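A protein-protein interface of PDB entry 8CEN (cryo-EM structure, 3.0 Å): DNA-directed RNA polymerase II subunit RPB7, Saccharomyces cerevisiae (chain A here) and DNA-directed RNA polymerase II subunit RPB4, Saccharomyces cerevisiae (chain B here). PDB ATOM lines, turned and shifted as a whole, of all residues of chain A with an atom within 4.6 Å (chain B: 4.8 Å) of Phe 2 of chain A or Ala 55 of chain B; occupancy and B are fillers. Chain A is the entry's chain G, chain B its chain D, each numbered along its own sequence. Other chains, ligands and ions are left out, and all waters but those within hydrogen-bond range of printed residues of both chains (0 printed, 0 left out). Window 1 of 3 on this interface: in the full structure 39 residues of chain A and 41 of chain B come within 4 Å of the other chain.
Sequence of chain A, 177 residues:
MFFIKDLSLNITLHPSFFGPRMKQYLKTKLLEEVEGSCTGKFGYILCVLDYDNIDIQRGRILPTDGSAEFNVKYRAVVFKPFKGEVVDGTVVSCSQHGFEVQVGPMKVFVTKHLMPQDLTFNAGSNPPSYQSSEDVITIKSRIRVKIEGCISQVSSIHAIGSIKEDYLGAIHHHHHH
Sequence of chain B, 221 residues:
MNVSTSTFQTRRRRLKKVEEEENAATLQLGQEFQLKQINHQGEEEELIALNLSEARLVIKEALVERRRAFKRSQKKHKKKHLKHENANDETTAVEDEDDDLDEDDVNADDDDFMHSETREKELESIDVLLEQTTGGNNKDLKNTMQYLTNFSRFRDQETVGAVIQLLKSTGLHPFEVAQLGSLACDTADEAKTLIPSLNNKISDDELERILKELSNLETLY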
ATOM      1  N   MET A   1      -2.439  -7.612   8.326  1.00  0.00           N
ATOM      2  CA  MET A   1      -2.585  -8.866   9.051  1.00  0.00           C
ATOM      3  C   MET A   1      -1.163  -9.379   9.291  1.00  0.00           C
ATOM      4  O   MET A   1      -0.219  -8.882   8.680  1.00  0.00           O
ATOM      5  CB  MET A   1      -3.440  -9.857   8.245  1.00  0.00           C
ATOM      6  CG  MET A   1      -3.748 -11.201   8.904  1.00  0.00           C
ATOM      7  SD  MET A   1      -4.768 -12.272   7.887  1.00  0.00           S
ATOM      8  CE  MET A   1      -3.573 -12.722   6.638  1.00  0.00           C
ATOM      9  N   PHE A   2      -0.998 -10.344  10.191  1.00  0.00           N
ATOM     10  CA  PHE A   2       0.318 -10.893  10.473  1.00  0.00           C
ATOM     11  C   PHE A   2       0.775 -11.798   9.332  1.00  0.00           C
ATOM     12  O   PHE A   2       0.026 -12.666   8.875  1.00  0.00           O
ATOM     13  CB  PHE A   2       0.285 -11.661  11.792  1.00  0.00           C
ATOM     14  CG  PHE A   2      -0.121 -10.816  12.966  1.00  0.00           C
ATOM     15  CD1 PHE A   2       0.819 -10.083  13.670  1.00  0.00           C
ATOM     16  CD2 PHE A   2      -1.449 -10.744  13.357  1.00  0.00           C
ATOM     17  CE1 PHE A   2       0.441  -9.300  14.746  1.00  0.00           C
ATOM     18  CE2 PHE A   2      -1.829  -9.961  14.429  1.00  0.00           C
ATOM     19  CZ  PHE A   2      -0.882  -9.239  15.123  1.00  0.00           C
ATOM     20  N   PHE A   3       2.006 -11.583   8.870  1.00  0.00           N
ATOM     21  CA  PHE A   3       2.620 -12.398   7.829  1.00  0.00           C
ATOM     22  C   PHE A   3       4.041 -12.745   8.244  1.00  0.00           C
ATOM     23  O   PHE A   3       4.585 -12.195   9.203  1.00  0.00           O
ATOM     24  CB  PHE A   3       2.665 -11.684   6.471  1.00  0.00           C
ATOM     25  CG  PHE A   3       1.327 -11.485   5.830  1.00  0.00           C
ATOM     26  CD1 PHE A   3       0.785 -12.460   5.010  1.00  0.00           C
ATOM     27  CD2 PHE A   3       0.629 -10.305   6.010  1.00  0.00           C
ATOM     28  CE1 PHE A   3      -0.442 -12.272   4.405  1.00  0.00           C
ATOM     29  CE2 PHE A   3      -0.598 -10.111   5.410  1.00  0.00           C
ATOM     30  CZ  PHE A   3      -1.132 -11.093   4.604  1.00  0.00           C
ATOM     31  N   LEU A  46       7.619  -6.720  13.326  1.00  0.00           N
ATOM     32  CA  LEU A  46       7.473  -6.896  14.767  1.00  0.00           C
ATOM     33  C   LEU A  46       8.673  -7.593  15.400  1.00  0.00           C
ATOM     34  O   LEU A  46       9.337  -7.025  16.272  1.00  0.00           O
ATOM     35  CB  LEU A  46       6.186  -7.677  15.053  1.00  0.00           C
ATOM     36  CG  LEU A  46       4.956  -7.196  14.280  1.00  0.00           C
ATOM     37  CD1 LEU A  46       3.749  -8.015  14.673  1.00  0.00           C
ATOM     38  CD2 LEU A  46       4.695  -5.709  14.499  1.00  0.00           C
ATOM     39  N   VAL A  78       5.684  -9.684  10.189  1.00  0.00           N
ATOM     40  CA  VAL A  78       5.264  -8.336   9.841  1.00  0.00           C
ATOM     41  C   VAL A  78       3.765  -8.212  10.088  1.00  0.00           C
ATOM     42  O   VAL A  78       3.071  -9.193  10.342  1.00  0.00           O
ATOM     43  CB  VAL A  78       5.609  -7.963   8.385  1.00  0.00           C
ATOM     44  CG1 VAL A  78       7.074  -8.245   8.085  1.00  0.00           C
ATOM     45  CG2 VAL A  78       4.712  -8.711   7.417  1.00  0.00           C
ATOM     46  N   PHE A  79       3.273  -6.975  10.020  1.00  0.00           N
ATOM     47  CA  PHE A  79       1.845  -6.686  10.167  1.00  0.00           C
ATOM     48  C   PHE A  79       1.488  -5.605   9.151  1.00  0.00           C
ATOM     49  O   PHE A  79       1.785  -4.426   9.364  1.00  0.00           O
ATOM     50  CB  PHE A  79       1.506  -6.250  11.588  1.00  0.00           C
ATOM     51  CG  PHE A  79       0.042  -5.991  11.810  1.00  0.00           C
ATOM     52  CD1 PHE A  79      -0.828  -7.039  12.060  1.00  0.00           C
ATOM     53  CD2 PHE A  79      -0.463  -4.701  11.771  1.00  0.00           C
ATOM     54  CE1 PHE A  79      -2.175  -6.807  12.265  1.00  0.00           C
ATOM     55  CE2 PHE A  79      -1.809  -4.462  11.974  1.00  0.00           C
ATOM     56  CZ  PHE A  79      -2.665  -5.517  12.222  1.00  0.00           C
ATOM     57  N   ILE B  48       3.229 -17.139   3.682  1.00  0.00           N
ATOM     58  CA  ILE B  48       2.920 -17.564   5.041  1.00  0.00           C
ATOM     59  C   ILE B  48       2.060 -16.483   5.684  1.00  0.00           C
ATOM     60  O   ILE B  48       2.553 -15.407   6.035  1.00  0.00           O
ATOM     61  CB  ILE B  48       4.197 -17.823   5.851  1.00  0.00           C
ATOM     62  CG1 ILE B  48       4.993 -18.970   5.228  1.00  0.00           C
ATOM     63  CG2 ILE B  48       3.854 -18.169   7.286  1.00  0.00           C
ATOM     64  CD1 ILE B  48       6.385 -19.128   5.801  1.00  0.00           C
ATOM     65  N   ALA B  49       0.769 -16.765   5.826  1.00  0.00           N
ATOM     66  CA  ALA B  49      -0.176 -15.869   6.475  1.00  0.00           C
ATOM     67  C   ALA B  49      -0.609 -16.488   7.795  1.00  0.00           C
ATOM     68  O   ALA B  49      -1.053 -17.640   7.829  1.00  0.00           O
ATOM     69  CB  ALA B  49      -1.390 -15.606   5.583  1.00  0.00           C
ATOM     70  N   LEU B  50      -0.483 -15.723   8.874  1.00  0.00           N
ATOM     71  CA  LEU B  50      -0.733 -16.216  10.219  1.00  0.00           C
ATOM     72  C   LEU B  50      -2.034 -15.648  10.766  1.00  0.00           C
ATOM     73  O   LEU B  50      -2.356 -14.476  10.542  1.00  0.00           O
ATOM     74  CB  LEU B  50       0.411 -15.844  11.165  1.00  0.00           C
ATOM     75  CG  LEU B  50       1.838 -16.197  10.753  1.00  0.00           C
ATOM     76  CD1 LEU B  50       2.800 -15.814  11.862  1.00  0.00           C
ATOM     77  CD2 LEU B  50       1.950 -17.673  10.434  1.00  0.00           C
ATOM     78  N   ASN B  51      -2.775 -16.483  11.489  1.00  0.00           N
ATOM     79  CA  ASN B  51      -3.856 -15.993  12.326  1.00  0.00           C
ATOM     80  C   ASN B  51      -3.270 -15.395  13.603  1.00  0.00           C
ATOM     81  O   ASN B  51      -2.055 -15.385  13.813  1.00  0.00           O
ATOM     82  CB  ASN B  51      -4.855 -17.109  12.624  1.00  0.00           C
ATOM     83  CG  ASN B  51      -4.210 -18.311  13.280  1.00  0.00           C
ATOM     84  OD1 ASN B  51      -4.041 -18.351  14.499  1.00  0.00           O
ATOM     85  ND2 ASN B  51      -3.853 -19.303  12.475  1.00  0.00           N
ATOM     86  N   LEU B  52      -4.144 -14.883  14.473  1.00  0.00           N
ATOM     87  CA  LEU B  52      -3.674 -14.131  15.633  1.00  0.00           C
ATOM     88  C   LEU B  52      -3.004 -15.038  16.663  1.00  0.00           C
ATOM     89  O   LEU B  52      -1.918 -14.717  17.164  1.00  0.00           O
ATOM     90  CB  LEU B  52      -4.837 -13.358  16.258  1.00  0.00           C
ATOM     91  CG  LEU B  52      -5.017 -11.892  15.834  1.00  0.00           C
ATOM     92  CD1 LEU B  52      -4.992 -11.709  14.324  1.00  0.00           C
ATOM     93  CD2 LEU B  52      -6.304 -11.327  16.402  1.00  0.00           C
ATOM     94  N   SER B  53      -3.625 -16.177  16.980  1.00  0.00           N
ATOM     95  CA  SER B  53      -3.030 -17.110  17.935  1.00  0.00           C
ATOM     96  C   SER B  53      -1.744 -17.718  17.388  1.00  0.00           C
ATOM     97  O   SER B  53      -0.768 -17.894  18.130  1.00  0.00           O
ATOM     98  CB  SER B  53      -4.030 -18.209  18.288  1.00  0.00           C
ATOM     99  OG  SER B  53      -4.305 -19.016  17.158  1.00  0.00           O
ATOM    100  N   GLU B  54      -1.729 -18.044  16.092  1.00  0.00           N
ATOM    101  CA  GLU B  54      -0.520 -18.564  15.462  1.00  0.00           C
ATOM    102  C   GLU B  54       0.608 -17.543  15.499  1.00  0.00           C
ATOM    103  O   GLU B  54       1.757 -17.892  15.788  1.00  0.00           O
ATOM    104  CB  GLU B  54      -0.814 -18.974  14.022  1.00  0.00           C
ATOM    105  CG  GLU B  54       0.337 -19.680  13.333  1.00  0.00           C
ATOM    106  CD  GLU B  54      -0.035 -20.178  11.954  1.00  0.00           C
ATOM    107  OE1 GLU B  54      -1.181 -19.928  11.524  1.00  0.00           O
ATOM    108  OE2 GLU B  54       0.817 -20.813  11.296  1.00  0.00           O
ATOM    109  N   ALA B  55       0.293 -16.274  15.222  1.00  0.00           N
ATOM    110  CA  ALA B  55       1.301 -15.222  15.283  1.00  0.00           C
ATOM    111  C   ALA B  55       1.823 -15.041  16.701  1.00  0.00           C
ATOM    112  O   ALA B  55       3.025 -14.837  16.903  1.00  0.00           O
ATOM    113  CB  ALA B  55       0.725 -13.910  14.756  1.00  0.00           C
ATOM    114  N   ARG B  56       0.930 -15.124  17.692  1.00  0.00           N
ATOM    115  CA  ARG B  56       1.348 -15.019  19.087  1.00  0.00           C
ATOM    116  C   ARG B  56       2.297 -16.149  19.463  1.00  0.00           C
ATOM    117  O   ARG B  56       3.320 -15.924  20.120  1.00  0.00           O
ATOM    118  CB  ARG B  56       0.122 -15.011  20.001  1.00  0.00           C
ATOM    119  CG  ARG B  56       0.421 -14.643  21.445  1.00  0.00           C
ATOM    120  CD  ARG B  56      -0.791 -14.863  22.342  1.00  0.00           C
ATOM    121  NE  ARG B  56      -1.071 -16.272  22.599  1.00  0.00           N
ATOM    122  CZ  ARG B  56      -0.478 -16.991  23.542  1.00  0.00           C
ATOM    123  NH1 ARG B  56       0.453 -16.471  24.326  1.00  0.00           N
ATOM    124  NH2 ARG B  56      -0.834 -18.261  23.711  1.00  0.00           N
ATOM    125  N   LEU B  57       1.988 -17.374  19.026  1.00  0.00           N
ATOM    126  CA  LEU B  57       2.867 -18.494  19.353  1.00  0.00           C
ATOM    127  C   LEU B  57       4.199 -18.419  18.616  1.00  0.00           C
ATOM    128  O   LEU B  57       5.233 -18.767  19.196  1.00  0.00           O
ATOM    129  CB  LEU B  57       2.172 -19.827  19.074  1.00  0.00           C
ATOM    130  CG  LEU B  57       0.902 -20.138  19.870  1.00  0.00           C
ATOM    131  CD1 LEU B  57       0.673 -21.626  19.888  1.00  0.00           C
ATOM    132  CD2 LEU B  57       1.001 -19.625  21.295  1.00  0.00           C
ATOM    133  N   VAL B  58       4.208 -17.954  17.363  1.00  0.00           N
ATOM    134  CA  VAL B  58       5.470 -17.804  16.635  1.00  0.00           C
ATOM    135  C   VAL B  58       6.348 -16.737  17.284  1.00  0.00           C
ATOM    136  O   VAL B  58       7.558 -16.935  17.464  1.00  0.00           O
ATOM    137  CB  VAL B  58       5.212 -17.503  15.146  1.00  0.00           C
ATOM    138  CG1 VAL B  58       6.516 -17.235  14.428  1.00  0.00           C
ATOM    139  CG2 VAL B  58       4.545 -18.692  14.482  1.00  0.00           C
ATOM    140  N   ILE B  59       5.755 -15.598  17.659  1.00  0.00           N
ATOM    141  CA  ILE B  59       6.523 -14.537  18.305  1.00  0.00           C
ATOM    142  C   ILE B  59       7.041 -14.994  19.667  1.00  0.00           C
ATOM    143  O   ILE B  59       8.201 -14.737  20.018  1.00  0.00           O
ATOM    144  CB  ILE B  59       5.678 -13.252  18.410  1.00  0.00           C
ATOM    145  CG1 ILE B  59       5.408 -12.680  17.018  1.00  0.00           C
ATOM    146  CG2 ILE B  59       6.386 -12.200  19.246  1.00  0.00           C
ATOM    147  CD1 ILE B  59       4.527 -11.451  17.023  1.00  0.00           C
ATOM    148  N   TYR B 147      -2.054  -7.167  22.402  1.00  0.00           N
ATOM    149  CA  TYR B 147      -3.176  -7.392  21.498  1.00  0.00           C
ATOM    150  C   TYR B 147      -3.369  -8.872  21.202  1.00  0.00           C
ATOM    151  O   TYR B 147      -4.502  -9.358  21.150  1.00  0.00           O
ATOM    152  CB  TYR B 147      -2.952  -6.600  20.207  1.00  0.00           C
ATOM    153  CG  TYR B 147      -3.833  -6.997  19.043  1.00  0.00           C
ATOM    154  CD1 TYR B 147      -5.136  -6.528  18.944  1.00  0.00           C
ATOM    155  CD2 TYR B 147      -3.351  -7.811  18.024  1.00  0.00           C
ATOM    156  CE1 TYR B 147      -5.941  -6.880  17.878  1.00  0.00           C
ATOM    157  CE2 TYR B 147      -4.148  -8.167  16.954  1.00  0.00           C
ATOM    158  CZ  TYR B 147      -5.443  -7.698  16.887  1.00  0.00           C
ATOM    159  OH  TYR B 147      -6.240  -8.048  15.822  1.00  0.00           O
ATOM    160  N   LEU B 148      -2.273  -9.609  21.014  1.00  0.00           N
ATOM    161  CA  LEU B 148      -2.387 -11.028  20.703  1.00  0.00           C
ATOM    162  C   LEU B 148      -2.808 -11.839  21.922  1.00  0.00           C
ATOM    163  O   LEU B 148      -3.595 -12.784  21.795  1.00  0.00           O
ATOM    164  CB  LEU B 148      -1.070 -11.543  20.127  1.00  0.00           C
ATOM    165  CG  LEU B 148      -0.765 -11.035  18.717  1.00  0.00           C
ATOM    166  CD1 LEU B 148       0.607 -11.487  18.245  1.00  0.00           C
ATOM    167  CD2 LEU B 148      -1.843 -11.488  17.757  1.00  0.00           C
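The backbone carbonyl oxygen (O) of Phe 2 of chain A lies within hydrogen-bond range of the backbone NH (N) of Leu 50 of chain B (3.1 Å).
Ala 49 of chain B touches Met 1 of chain A.
Met 1 of chain A touches Leu 50 of chain B.
Leu 52 of chain B touches Phe 2 of chain A.
Phe 2 of chain A touches Ala 55 of chain B.
CE2 of Tyr 147 of chain B touches CE2 of Phe 2 of chain A, 3.9 Å away.
CZ of Phe 2 of chain A touches CD2 of Leu 148 of chain B (3.6 Å).
Phe 3 of chain A touches Ile 48 of chain B.
Ala 49 of chain B touches Phe 3 of chain A (CB to CE1, 3.7 Å).
The backbone carbonyl oxygen (O) of Phe 3 of chain A is in hydrogen-bond range of the backbone NH (N) of Val 78 of chain A (2.9 Å).
Printed residues of chain B within 4 Å of Phe 2 of chain A: Leu 50, Leu 52, Ala 55, Tyr 147 and Leu 148.
Leu 46 of chain A touches none of the printed residues of chain B.
Of the printed residues of chain A, Ile 48 of chain B touches Phe 3.
Printed residues of chain A within 4 Å of Leu 52 of chain B: Phe 2 (3.6 Å).
Ala 55 of chain B touches one residue of chain A.
Of the printed residues of chain A, Tyr 147 of chain B touches Phe 2 (3.9 Å).
Of the printed residues of chain A, Leu 148 of chain B touches Phe 2.
The nearest printed residue of chain B that does not touch Phe 2 of chain A is Ala 49 of chain B (4.01 Å).
The nearest printed residue of chain A that does not touch Leu 148 of chain B is Leu 46 of chain A (5.9 Å).
Of the 6 printed residues of chain A, 3 touch a printed residue of chain B.
Of the 14 printed residues of chain B, 7 touch a printed residue of chain A.
Hydrophobic or aromatic side chains of chain B within 4 Å of the printed part of chain A: Ala 49, Leu 50, Leu 52, Ala 55, Tyr 147 and Leu 148.
Among the printed residues, 9 pairs touch across the chains.
Among the printed residues, no Asp or Glu carboxylate lies within 4 Å of a Lys or Arg side-chain nitrogen of the other chain.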
